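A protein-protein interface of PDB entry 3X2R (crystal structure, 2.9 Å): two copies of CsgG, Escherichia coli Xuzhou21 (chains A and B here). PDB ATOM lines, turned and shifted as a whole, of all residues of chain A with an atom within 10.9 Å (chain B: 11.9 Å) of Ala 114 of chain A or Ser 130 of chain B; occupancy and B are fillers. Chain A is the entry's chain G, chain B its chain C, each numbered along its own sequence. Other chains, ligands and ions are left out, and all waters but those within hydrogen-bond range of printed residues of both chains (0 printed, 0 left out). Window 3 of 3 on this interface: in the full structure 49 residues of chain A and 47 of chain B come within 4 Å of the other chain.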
ATOM      1  N   ASN A 106       1.140  36.370  15.201  1.00  0.00           N
ATOM      2  CA  ASN A 106       1.471  34.967  14.994  1.00  0.00           C
ATOM      3  C   ASN A 106       2.941  34.711  15.325  1.00  0.00           C
ATOM      4  O   ASN A 106       3.280  33.758  16.033  1.00  0.00           O
ATOM      5  CB  ASN A 106       1.174  34.553  13.552  1.00  0.00           C
ATOM      6  CG  ASN A 106      -0.315  34.432  13.275  1.00  0.00           C
ATOM      7  OD1 ASN A 106      -1.099  34.163  14.187  1.00  0.00           O
ATOM      8  ND2 ASN A 106      -0.713  34.629  12.013  1.00  0.00           N
ATOM      9  N   GLU A 107       3.809  35.571  14.802  1.00  0.00           N
ATOM     10  CA  GLU A 107       5.241  35.461  15.037  1.00  0.00           C
ATOM     11  C   GLU A 107       5.572  35.488  16.523  1.00  0.00           C
ATOM     12  O   GLU A 107       6.408  34.716  17.008  1.00  0.00           O
ATOM     13  CB  GLU A 107       5.976  36.601  14.335  1.00  0.00           C
ATOM     14  CG  GLU A 107       7.477  36.375  14.211  1.00  0.00           C
ATOM     15  CD  GLU A 107       7.821  35.165  13.352  1.00  0.00           C
ATOM     16  OE1 GLU A 107       7.058  34.840  12.424  1.00  0.00           O
ATOM     17  OE2 GLU A 107       8.849  34.520  13.615  1.00  0.00           O
ATOM     18  N   ARG A 108       4.924  36.390  17.249  1.00  0.00           N
ATOM     19  CA  ARG A 108       5.125  36.454  18.688  1.00  0.00           C
ATOM     20  C   ARG A 108       4.570  35.211  19.383  1.00  0.00           C
ATOM     21  O   ARG A 108       5.090  34.802  20.423  1.00  0.00           O
ATOM     22  CB  ARG A 108       4.540  37.743  19.261  1.00  0.00           C
ATOM     23  CG  ARG A 108       5.288  39.002  18.815  1.00  0.00           C
ATOM     24  CD  ARG A 108       4.550  40.276  19.209  1.00  0.00           C
ATOM     25  NE  ARG A 108       4.455  40.477  20.649  1.00  0.00           N
ATOM     26  CZ  ARG A 108       5.307  41.207  21.357  1.00  0.00           C
ATOM     27  NH1 ARG A 108       6.324  41.808  20.753  1.00  0.00           N
ATOM     28  NH2 ARG A 108       5.144  41.334  22.668  1.00  0.00           N
ATOM     29  N   LYS A 109       3.524  34.611  18.806  1.00  0.00           N
ATOM     30  CA  LYS A 109       2.996  33.341  19.319  1.00  0.00           C
ATOM     31  C   LYS A 109       4.065  32.265  19.221  1.00  0.00           C
ATOM     32  O   LYS A 109       4.261  31.477  20.149  1.00  0.00           O
ATOM     33  CB  LYS A 109       1.759  32.875  18.546  1.00  0.00           C
ATOM     34  CG  LYS A 109       0.476  33.624  18.833  1.00  0.00           C
ATOM     35  CD  LYS A 109      -0.724  32.764  18.467  1.00  0.00           C
ATOM     36  CE  LYS A 109      -1.982  33.595  18.294  1.00  0.00           C
ATOM     37  NZ  LYS A 109      -1.975  34.362  17.015  1.00  0.00           N
ATOM     38  N   ILE A 110       4.736  32.230  18.074  1.00  0.00           N
ATOM     39  CA  ILE A 110       5.848  31.313  17.859  1.00  0.00           C
ATOM     40  C   ILE A 110       6.996  31.555  18.846  1.00  0.00           C
ATOM     41  O   ILE A 110       7.503  30.603  19.448  1.00  0.00           O
ATOM     42  CB  ILE A 110       6.372  31.402  16.415  1.00  0.00           C
ATOM     43  CG1 ILE A 110       5.378  30.752  15.452  1.00  0.00           C
ATOM     44  CG2 ILE A 110       7.739  30.740  16.294  1.00  0.00           C
ATOM     45  CD1 ILE A 110       5.270  31.466  14.134  1.00  0.00           C
ATOM     46  N   ILE A 111       7.395  32.818  19.016  1.00  0.00           N
ATOM     47  CA  ILE A 111       8.450  33.166  19.973  1.00  0.00           C
ATOM     48  C   ILE A 111       8.096  32.675  21.367  1.00  0.00           C
ATOM     49  O   ILE A 111       8.909  32.051  22.045  1.00  0.00           O
ATOM     50  CB  ILE A 111       8.684  34.689  20.062  1.00  0.00           C
ATOM     51  CG1 ILE A 111       9.172  35.251  18.728  1.00  0.00           C
ATOM     52  CG2 ILE A 111       9.693  35.017  21.158  1.00  0.00           C
ATOM     53  CD1 ILE A 111       9.690  36.674  18.823  1.00  0.00           C
ATOM     54  N   ARG A 112       6.875  32.980  21.792  1.00  0.00           N
ATOM     55  CA  ARG A 112       6.395  32.602  23.114  1.00  0.00           C
ATOM     56  C   ARG A 112       6.323  31.074  23.256  1.00  0.00           C
ATOM     57  O   ARG A 112       6.496  30.529  24.349  1.00  0.00           O
ATOM     58  CB  ARG A 112       5.028  33.252  23.375  1.00  0.00           C
ATOM     59  CG  ARG A 112       4.674  33.424  24.847  1.00  0.00           C
ATOM     60  CD  ARG A 112       3.420  34.282  25.053  1.00  0.00           C
ATOM     61  NE  ARG A 112       3.609  35.686  24.680  1.00  0.00           N
ATOM     62  CZ  ARG A 112       3.135  36.243  23.569  1.00  0.00           C
ATOM     63  NH1 ARG A 112       2.442  35.520  22.700  1.00  0.00           N
ATOM     64  NH2 ARG A 112       3.357  37.528  23.325  1.00  0.00           N
ATOM     65  N   ALA A 113       6.078  30.390  22.142  1.00  0.00           N
ATOM     66  CA  ALA A 113       5.994  28.933  22.142  1.00  0.00           C
ATOM     67  C   ALA A 113       7.358  28.260  22.269  1.00  0.00           C
ATOM     68  O   ALA A 113       7.506  27.268  22.984  1.00  0.00           O
ATOM     69  CB  ALA A 113       5.299  28.454  20.885  1.00  0.00           C
ATOM     70  N   ALA A 114       8.353  28.811  21.580  1.00  0.00           N
ATOM     71  CA  ALA A 114       9.694  28.233  21.565  1.00  0.00           C
ATOM     72  C   ALA A 114      10.376  28.344  22.926  1.00  0.00           C
ATOM     73  O   ALA A 114      11.355  27.648  23.204  1.00  0.00           O
ATOM     74  CB  ALA A 114      10.538  28.891  20.489  1.00  0.00           C
ATOM     75  N   GLN A 115       9.846  29.226  23.768  1.00  0.00           N
ATOM     76  CA  GLN A 115      10.409  29.489  25.089  1.00  0.00           C
ATOM     77  C   GLN A 115       9.749  28.646  26.180  1.00  0.00           C
ATOM     78  O   GLN A 115      10.079  28.775  27.359  1.00  0.00           O
ATOM     79  CB  GLN A 115      10.290  30.976  25.424  1.00  0.00           C
ATOM     80  CG  GLN A 115      11.116  31.881  24.524  1.00  0.00           C
ATOM     81  CD  GLN A 115      10.904  33.351  24.829  1.00  0.00           C
ATOM     82  OE1 GLN A 115      10.052  33.708  25.641  1.00  0.00           O
ATOM     83  NE2 GLN A 115      11.675  34.212  24.174  1.00  0.00           N
ATOM     84  N   GLU A 116       8.818  27.784  25.779  1.00  0.00           N
ATOM     85  CA  GLU A 116       8.124  26.909  26.717  1.00  0.00           C
ATOM     86  C   GLU A 116       8.192  25.451  26.273  1.00  0.00           C
ATOM     87  O   GLU A 116       9.002  24.674  26.781  1.00  0.00           O
ATOM     88  CB  GLU A 116       6.664  27.339  26.874  1.00  0.00           C
ATOM     89  N   PHE B  50      17.389  35.799  11.277  1.00  0.00           N
ATOM     90  CA  PHE B  50      16.192  35.043  10.893  1.00  0.00           C
ATOM     91  C   PHE B  50      15.067  35.992  10.477  1.00  0.00           C
ATOM     92  O   PHE B  50      14.542  36.756  11.290  1.00  0.00           O
ATOM     93  CB  PHE B  50      15.721  34.211  12.084  1.00  0.00           C
ATOM     94  CG  PHE B  50      16.622  33.061  12.411  1.00  0.00           C
ATOM     95  CD1 PHE B  50      17.024  32.174  11.424  1.00  0.00           C
ATOM     96  CD2 PHE B  50      17.117  32.899  13.694  1.00  0.00           C
ATOM     97  CE1 PHE B  50      17.857  31.116  11.721  1.00  0.00           C
ATOM     98  CE2 PHE B  50      17.956  31.847  13.995  1.00  0.00           C
ATOM     99  CZ  PHE B  50      18.327  30.953  13.006  1.00  0.00           C
ATOM    100  N   LEU B  96      12.283  32.506   6.981  1.00  0.00           N
ATOM    101  CA  LEU B  96      11.617  31.620   7.928  1.00  0.00           C
ATOM    102  C   LEU B  96      10.334  30.900   7.478  1.00  0.00           C
ATOM    103  O   LEU B  96       9.636  30.333   8.317  1.00  0.00           O
ATOM    104  CB  LEU B  96      11.443  32.322   9.277  1.00  0.00           C
ATOM    105  CG  LEU B  96      12.280  31.724  10.406  1.00  0.00           C
ATOM    106  CD1 LEU B  96      11.565  30.551  10.995  1.00  0.00           C
ATOM    107  CD2 LEU B  96      13.612  31.272   9.866  1.00  0.00           C
ATOM    108  N   ARG B  98       6.586  30.639   6.787  1.00  0.00           N
ATOM    109  CA  ARG B  98       5.346  31.283   7.241  1.00  0.00           C
ATOM    110  C   ARG B  98       4.404  31.624   6.092  1.00  0.00           C
ATOM    111  O   ARG B  98       3.564  32.506   6.224  1.00  0.00           O
ATOM    112  CB  ARG B  98       5.624  32.563   8.062  1.00  0.00           C
ATOM    113  CG  ARG B  98       5.954  32.345   9.526  1.00  0.00           C
ATOM    114  CD  ARG B  98       7.356  31.829   9.694  1.00  0.00           C
ATOM    115  NE  ARG B  98       7.495  30.994  10.880  1.00  0.00           N
ATOM    116  CZ  ARG B  98       8.159  31.357  11.971  1.00  0.00           C
ATOM    117  NH1 ARG B  98       8.749  32.542  12.026  1.00  0.00           N
ATOM    118  NH2 ARG B  98       8.239  30.534  13.004  1.00  0.00           N
ATOM    119  N   LEU B 101       2.763  28.366   6.336  1.00  0.00           N
ATOM    120  CA  LEU B 101       2.842  27.920   7.730  1.00  0.00           C
ATOM    121  C   LEU B 101       1.887  26.762   8.057  1.00  0.00           C
ATOM    122  O   LEU B 101       2.242  25.847   8.806  1.00  0.00           O
ATOM    123  CB  LEU B 101       2.549  29.091   8.668  1.00  0.00           C
ATOM    124  CG  LEU B 101       3.333  29.234   9.975  1.00  0.00           C
ATOM    125  CD1 LEU B 101       2.673  30.277  10.853  1.00  0.00           C
ATOM    126  CD2 LEU B 101       3.483  27.937  10.735  1.00  0.00           C
ATOM    127  N   LEU B 104       3.070  23.288   7.173  1.00  0.00           N
ATOM    128  CA  LEU B 104       4.179  22.967   8.065  1.00  0.00           C
ATOM    129  C   LEU B 104       3.636  22.474   9.403  1.00  0.00           C
ATOM    130  O   LEU B 104       4.127  21.494   9.986  1.00  0.00           O
ATOM    131  CB  LEU B 104       5.045  24.215   8.278  1.00  0.00           C
ATOM    132  CG  LEU B 104       6.530  24.073   8.643  1.00  0.00           C
ATOM    133  CD1 LEU B 104       7.275  25.369   8.337  1.00  0.00           C
ATOM    134  CD2 LEU B 104       6.734  23.678  10.088  1.00  0.00           C
ATOM    135  N   LEU B 105       2.589  23.144   9.867  1.00  0.00           N
ATOM    136  CA  LEU B 105       1.980  22.815  11.144  1.00  0.00           C
ATOM    137  C   LEU B 105       1.311  21.450  11.074  1.00  0.00           C
ATOM    138  O   LEU B 105       1.369  20.684  12.036  1.00  0.00           O
ATOM    139  CB  LEU B 105       0.968  23.889  11.535  1.00  0.00           C
ATOM    140  CG  LEU B 105       1.615  25.170  12.056  1.00  0.00           C
ATOM    141  CD1 LEU B 105       0.573  26.146  12.508  1.00  0.00           C
ATOM    142  CD2 LEU B 105       2.586  24.863  13.185  1.00  0.00           C
ATOM    143  N   GLU B 107       2.205  18.919   8.920  1.00  0.00           N
ATOM    144  CA  GLU B 107       3.276  17.939   8.840  1.00  0.00           C
ATOM    145  C   GLU B 107       3.825  17.663  10.230  1.00  0.00           C
ATOM    146  O   GLU B 107       4.130  16.517  10.571  1.00  0.00           O
ATOM    147  CB  GLU B 107       4.389  18.429   7.928  1.00  0.00           C
ATOM    148  CG  GLU B 107       5.333  17.331   7.488  1.00  0.00           C
ATOM    149  CD  GLU B 107       4.626  16.265   6.676  1.00  0.00           C
ATOM    150  OE1 GLU B 107       3.617  16.586   6.016  1.00  0.00           O
ATOM    151  OE2 GLU B 107       5.083  15.105   6.683  1.00  0.00           O
ATOM    152  N   ARG B 108       3.974  18.720  11.026  1.00  0.00           N
ATOM    153  CA  ARG B 108       4.394  18.537  12.413  1.00  0.00           C
ATOM    154  C   ARG B 108       3.328  17.808  13.240  1.00  0.00           C
ATOM    155  O   ARG B 108       3.664  17.111  14.200  1.00  0.00           O
ATOM    156  CB  ARG B 108       4.805  19.865  13.059  1.00  0.00           C
ATOM    157  CG  ARG B 108       6.114  20.452  12.519  1.00  0.00           C
ATOM    158  CD  ARG B 108       6.348  21.869  13.034  1.00  0.00           C
ATOM    159  NE  ARG B 108       6.529  21.944  14.482  1.00  0.00           N
ATOM    160  CZ  ARG B 108       7.708  21.948  15.094  1.00  0.00           C
ATOM    161  NH1 ARG B 108       8.825  21.884  14.385  1.00  0.00           N
ATOM    162  NH2 ARG B 108       7.772  22.022  16.417  1.00  0.00           N
ATOM    163  N   LYS B 109       2.053  17.975  12.876  1.00  0.00           N
ATOM    164  CA  LYS B 109       0.978  17.206  13.513  1.00  0.00           C
ATOM    165  C   LYS B 109       1.174  15.716  13.234  1.00  0.00           C
ATOM    166  O   LYS B 109       1.058  14.884  14.138  1.00  0.00           O
ATOM    167  CB  LYS B 109      -0.409  17.644  13.020  1.00  0.00           C
ATOM    168  CG  LYS B 109      -0.910  18.964  13.579  1.00  0.00           C
ATOM    169  CD  LYS B 109      -2.429  19.052  13.481  1.00  0.00           C
ATOM    170  CE  LYS B 109      -2.945  20.481  13.647  1.00  0.00           C
ATOM    171  NZ  LYS B 109      -2.723  21.352  12.457  1.00  0.00           N
ATOM    172  N   ILE B 111       4.072  14.200  12.350  1.00  0.00           N
ATOM    173  CA  ILE B 111       5.280  13.775  13.055  1.00  0.00           C
ATOM    174  C   ILE B 111       4.998  13.499  14.520  1.00  0.00           C
ATOM    175  O   ILE B 111       5.304  12.421  15.031  1.00  0.00           O
ATOM    176  CB  ILE B 111       6.389  14.847  13.013  1.00  0.00           C
ATOM    177  CG1 ILE B 111       6.840  15.127  11.581  1.00  0.00           C
ATOM    178  CG2 ILE B 111       7.580  14.415  13.866  1.00  0.00           C
ATOM    179  CD1 ILE B 111       8.113  15.949  11.500  1.00  0.00           C
ATOM    180  N   ARG B 112       4.389  14.474  15.184  1.00  0.00           N
ATOM    181  CA  ARG B 112       4.105  14.367  16.606  1.00  0.00           C
ATOM    182  C   ARG B 112       3.147  13.209  16.876  1.00  0.00           C
ATOM    183  O   ARG B 112       3.205  12.583  17.934  1.00  0.00           O
ATOM    184  CB  ARG B 112       3.522  15.678  17.134  1.00  0.00           C
ATOM    185  CG  ARG B 112       3.719  15.890  18.622  1.00  0.00           C
ATOM    186  CD  ARG B 112       3.298  17.293  19.052  1.00  0.00           C
ATOM    187  NE  ARG B 112       4.144  18.339  18.482  1.00  0.00           N
ATOM    188  CZ  ARG B 112       3.778  19.135  17.482  1.00  0.00           C
ATOM    189  NH1 ARG B 112       2.573  19.011  16.938  1.00  0.00           N
ATOM    190  NH2 ARG B 112       4.615  20.060  17.029  1.00  0.00           N
ATOM    191  N   GLN B 115       4.938   9.577  16.731  1.00  0.00           N
ATOM    192  CA  GLN B 115       5.876   9.290  17.814  1.00  0.00           C
ATOM    193  C   GLN B 115       5.192   9.004  19.152  1.00  0.00           C
ATOM    194  O   GLN B 115       5.859   8.804  20.167  1.00  0.00           O
ATOM    195  CB  GLN B 115       6.890  10.426  17.949  1.00  0.00           C
ATOM    196  CG  GLN B 115       7.813  10.552  16.747  1.00  0.00           C
ATOM    197  CD  GLN B 115       8.765  11.724  16.859  1.00  0.00           C
ATOM    198  OE1 GLN B 115       8.672  12.529  17.787  1.00  0.00           O
ATOM    199  NE2 GLN B 115       9.685  11.831  15.906  1.00  0.00           N
ATOM    200  N   GLN B 129      12.621  19.517  17.604  1.00  0.00           N
ATOM    201  CA  GLN B 129      11.291  19.306  18.161  1.00  0.00           C
ATOM    202  C   GLN B 129      10.707  20.614  18.694  1.00  0.00           C
ATOM    203  O   GLN B 129       9.809  20.614  19.535  1.00  0.00           O
ATOM    204  CB  GLN B 129      11.311  18.213  19.236  1.00  0.00           C
ATOM    205  CG  GLN B 129      11.750  16.848  18.700  1.00  0.00           C
ATOM    206  CD  GLN B 129      11.990  15.817  19.791  1.00  0.00           C
ATOM    207  OE1 GLN B 129      11.530  15.970  20.923  1.00  0.00           O
ATOM    208  NE2 GLN B 129      12.703  14.749  19.447  1.00  0.00           N
ATOM    209  N   SER B 130      11.253  21.728  18.215  1.00  0.00           N
ATOM    210  CA  SER B 130      10.657  23.044  18.436  1.00  0.00           C
ATOM    211  C   SER B 130      10.748  23.880  17.162  1.00  0.00           C
ATOM    212  O   SER B 130      11.309  23.433  16.168  1.00  0.00           O
ATOM    213  CB  SER B 130      11.308  23.774  19.598  1.00  0.00           C
ATOM    214  OG  SER B 130      10.888  25.121  19.595  1.00  0.00           O
ATOM    215  N   LEU B 131      10.210  25.094  17.191  1.00  0.00           N
ATOM    216  CA  LEU B 131       9.978  25.832  15.953  1.00  0.00           C
ATOM    217  C   LEU B 131      10.621  27.209  16.010  1.00  0.00           C
ATOM    218  O   LEU B 131      10.206  28.060  16.794  1.00  0.00           O
ATOM    219  CB  LEU B 131       8.469  25.979  15.720  1.00  0.00           C
ATOM    220  CG  LEU B 131       7.983  26.270  14.298  1.00  0.00           C
ATOM    221  CD1 LEU B 131       8.561  25.264  13.310  1.00  0.00           C
ATOM    222  CD2 LEU B 131       6.463  26.288  14.230  1.00  0.00           C
ATOM    223  N   THR B 132      11.627  27.438  15.173  1.00  0.00           N
ATOM    224  CA  THR B 132      12.421  28.662  15.284  1.00  0.00           C
ATOM    225  C   THR B 132      11.639  29.907  14.884  1.00  0.00           C
ATOM    226  O   THR B 132      10.868  29.892  13.933  1.00  0.00           O
ATOM    227  CB  THR B 132      13.740  28.582  14.473  1.00  0.00           C
ATOM    228  OG1 THR B 132      13.504  28.946  13.108  1.00  0.00           O
ATOM    229  CG2 THR B 132      14.319  27.182  14.538  1.00  0.00           C
ATOM    230  N   ALA B 133      11.849  30.987  15.624  1.00  0.00           N
ATOM    231  CA  ALA B 133      11.154  32.237  15.361  1.00  0.00           C
ATOM    232  C   ALA B 133      12.041  33.155  14.541  1.00  0.00           C
ATOM    233  O   ALA B 133      13.189  32.824  14.252  1.00  0.00           O
ATOM    234  CB  ALA B 133      10.772  32.907  16.663  1.00  0.00           C
ATOM    235  N   ALA B 134      11.517  34.318  14.182  1.00  0.00           N
ATOM    236  CA  ALA B 134      12.290  35.267  13.398  1.00  0.00           C
ATOM    237  C   ALA B 134      12.367  36.563  14.154  1.00  0.00           C
ATOM    238  O   ALA B 134      11.354  37.067  14.629  1.00  0.00           O
ATOM    239  CB  ALA B 134      11.663  35.486  12.059  1.00  0.00           C
ATOM    240  N   ASN B 135      13.569  37.117  14.239  1.00  0.00           N
ATOM    241  CA  ASN B 135      13.779  38.307  15.042  1.00  0.00           C
ATOM    242  C   ASN B 135      13.398  39.598  14.301  1.00  0.00           C
ATOM    243  O   ASN B 135      13.094  40.624  14.924  1.00  0.00           O
ATOM    244  CB  ASN B 135      15.228  38.334  15.543  1.00  0.00           C
ATOM    245  CG  ASN B 135      15.348  38.885  16.948  1.00  0.00           C
ATOM    246  OD1 ASN B 135      14.568  39.746  17.367  1.00  0.00           O
ATOM    247  ND2 ASN B 135      16.314  38.362  17.700  1.00  0.00           N
ATOM    248  N   VAL B 181      10.286  42.615  15.424  1.00  0.00           N
ATOM    249  CA  VAL B 181       9.358  41.650  15.997  1.00  0.00           C
ATOM    250  C   VAL B 181       9.080  41.869  17.488  1.00  0.00           C
ATOM    251  O   VAL B 181       7.949  41.696  17.944  1.00  0.00           O
ATOM    252  CB  VAL B 181       9.823  40.204  15.732  1.00  0.00           C
ATOM    253  CG1 VAL B 181       8.924  39.203  16.429  1.00  0.00           C
ATOM    254  CG2 VAL B 181       9.856  39.943  14.239  1.00  0.00           C
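OE2 of Glu 107 of chain A lies within salt-bridge range of NH1 of Arg 98 of chain B, at 2.5 Å. The backbone NH (N) of Ala 134 of chain B sits at hydrogen-bond distance from the side-chain carboxylate (OE2) of Glu 107 of chain A (2.7 Å). The backbone carbonyl oxygen (O) of Val 181 of chain B lies within hydrogen-bond range of the guanidinium group (NH1) of Arg 108 of chain A.
The backbone carbonyl oxygen (O) of Leu 96 of chain B sits close to the guanidinium group (NE) of Arg 98 of chain B (3.4 Å). The guanidinium group (NH2) of Arg 98 of chain B sits at hydrogen-bond distance from the backbone carbonyl oxygen (O) of Thr 132 of chain B. The guanidinium group (NH1) of Arg 108 of chain B lies within hydrogen-bond range of the backbone carbonyl oxygen (O) of Ser 130 of chain B (3.4 Å). The backbone carbonyl oxygen (O) of Asn 135 of chain B sits close to the backbone NH (N) of Val 181 of chain B, at 3.5 Å.
Among the printed residues, pairs that only touch across the chains: Ile 110 of chain A with Arg 98 of chain B (3.3 Å), Ile 111 of chain A with Ala 133 of chain B (3.5 Å), Ile 111 of chain A with Val 181 of chain B (3.6 Å), Glu 107 of chain A with Ala 133 of chain B (3.6 Å), Ile 110 of chain A with Leu 131 of chain B (3.7 Å), Ile 110 of chain A with Ala 133 of chain B (3.7 Å), Ala 114 of chain A with Leu 131 of chain B (3.8 Å), Ala 114 of chain A with Ser 130 of chain B (3.9 Å) and Glu 107 of chain A with Val 181 of chain B (3.9 Å).
Asn 106 of chain A touches none of the printed residues of chain B. Of the printed residues of chain B, Glu 107 of chain A touches Arg 98 (2.5 Å), Ala 133 (3.6 Å), Ala 134 (2.7 Å) and Val 181 (3.9 Å). Ala 114 of chain A touches just these residues of chain B: Ser 130 (3.9 Å) and Leu 131 (3.8 Å). No residue of chain B comes within 4 Å of Gln 115 of chain A. No residue of chain B comes within 4 Å of Glu 116 of chain A. Arg 112 of chain B touches none of the printed residues of chain A. Ser 130 of chain B touches one residue of chain A. Of the printed residues of chain A, Ala 133 of chain B touches Glu 107 (3.6 Å), Ile 110 (3.7 Å) and Ile 111 (3.5 Å).
Of the 20 printed residues of chain B, 6 touch a printed residue of chain A. Hydrophobic or aromatic side chains of chain B within 4 Å of the printed part of chain A: Ala 133, Ala 134 and Val 181. Hydrophobic or aromatic side chains of chain A within 4 Å of the printed part of chain B: Ile 110, Ile 111 and Ala 114. Among the printed residues, 12 pairs touch across the chains. Among the printed residues, Asp or Glu carboxylates within 4 Å of a Lys or Arg side-chain nitrogen of the other chain: Glu 107 of chain A with Arg 98 of chain B.
Positions printed for both chains: 107, 108, 109, 111, 112 and 115. Of the 12 pairs that touch across the chains among the printed residues, none has its exchanged pair printed and touching as well.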
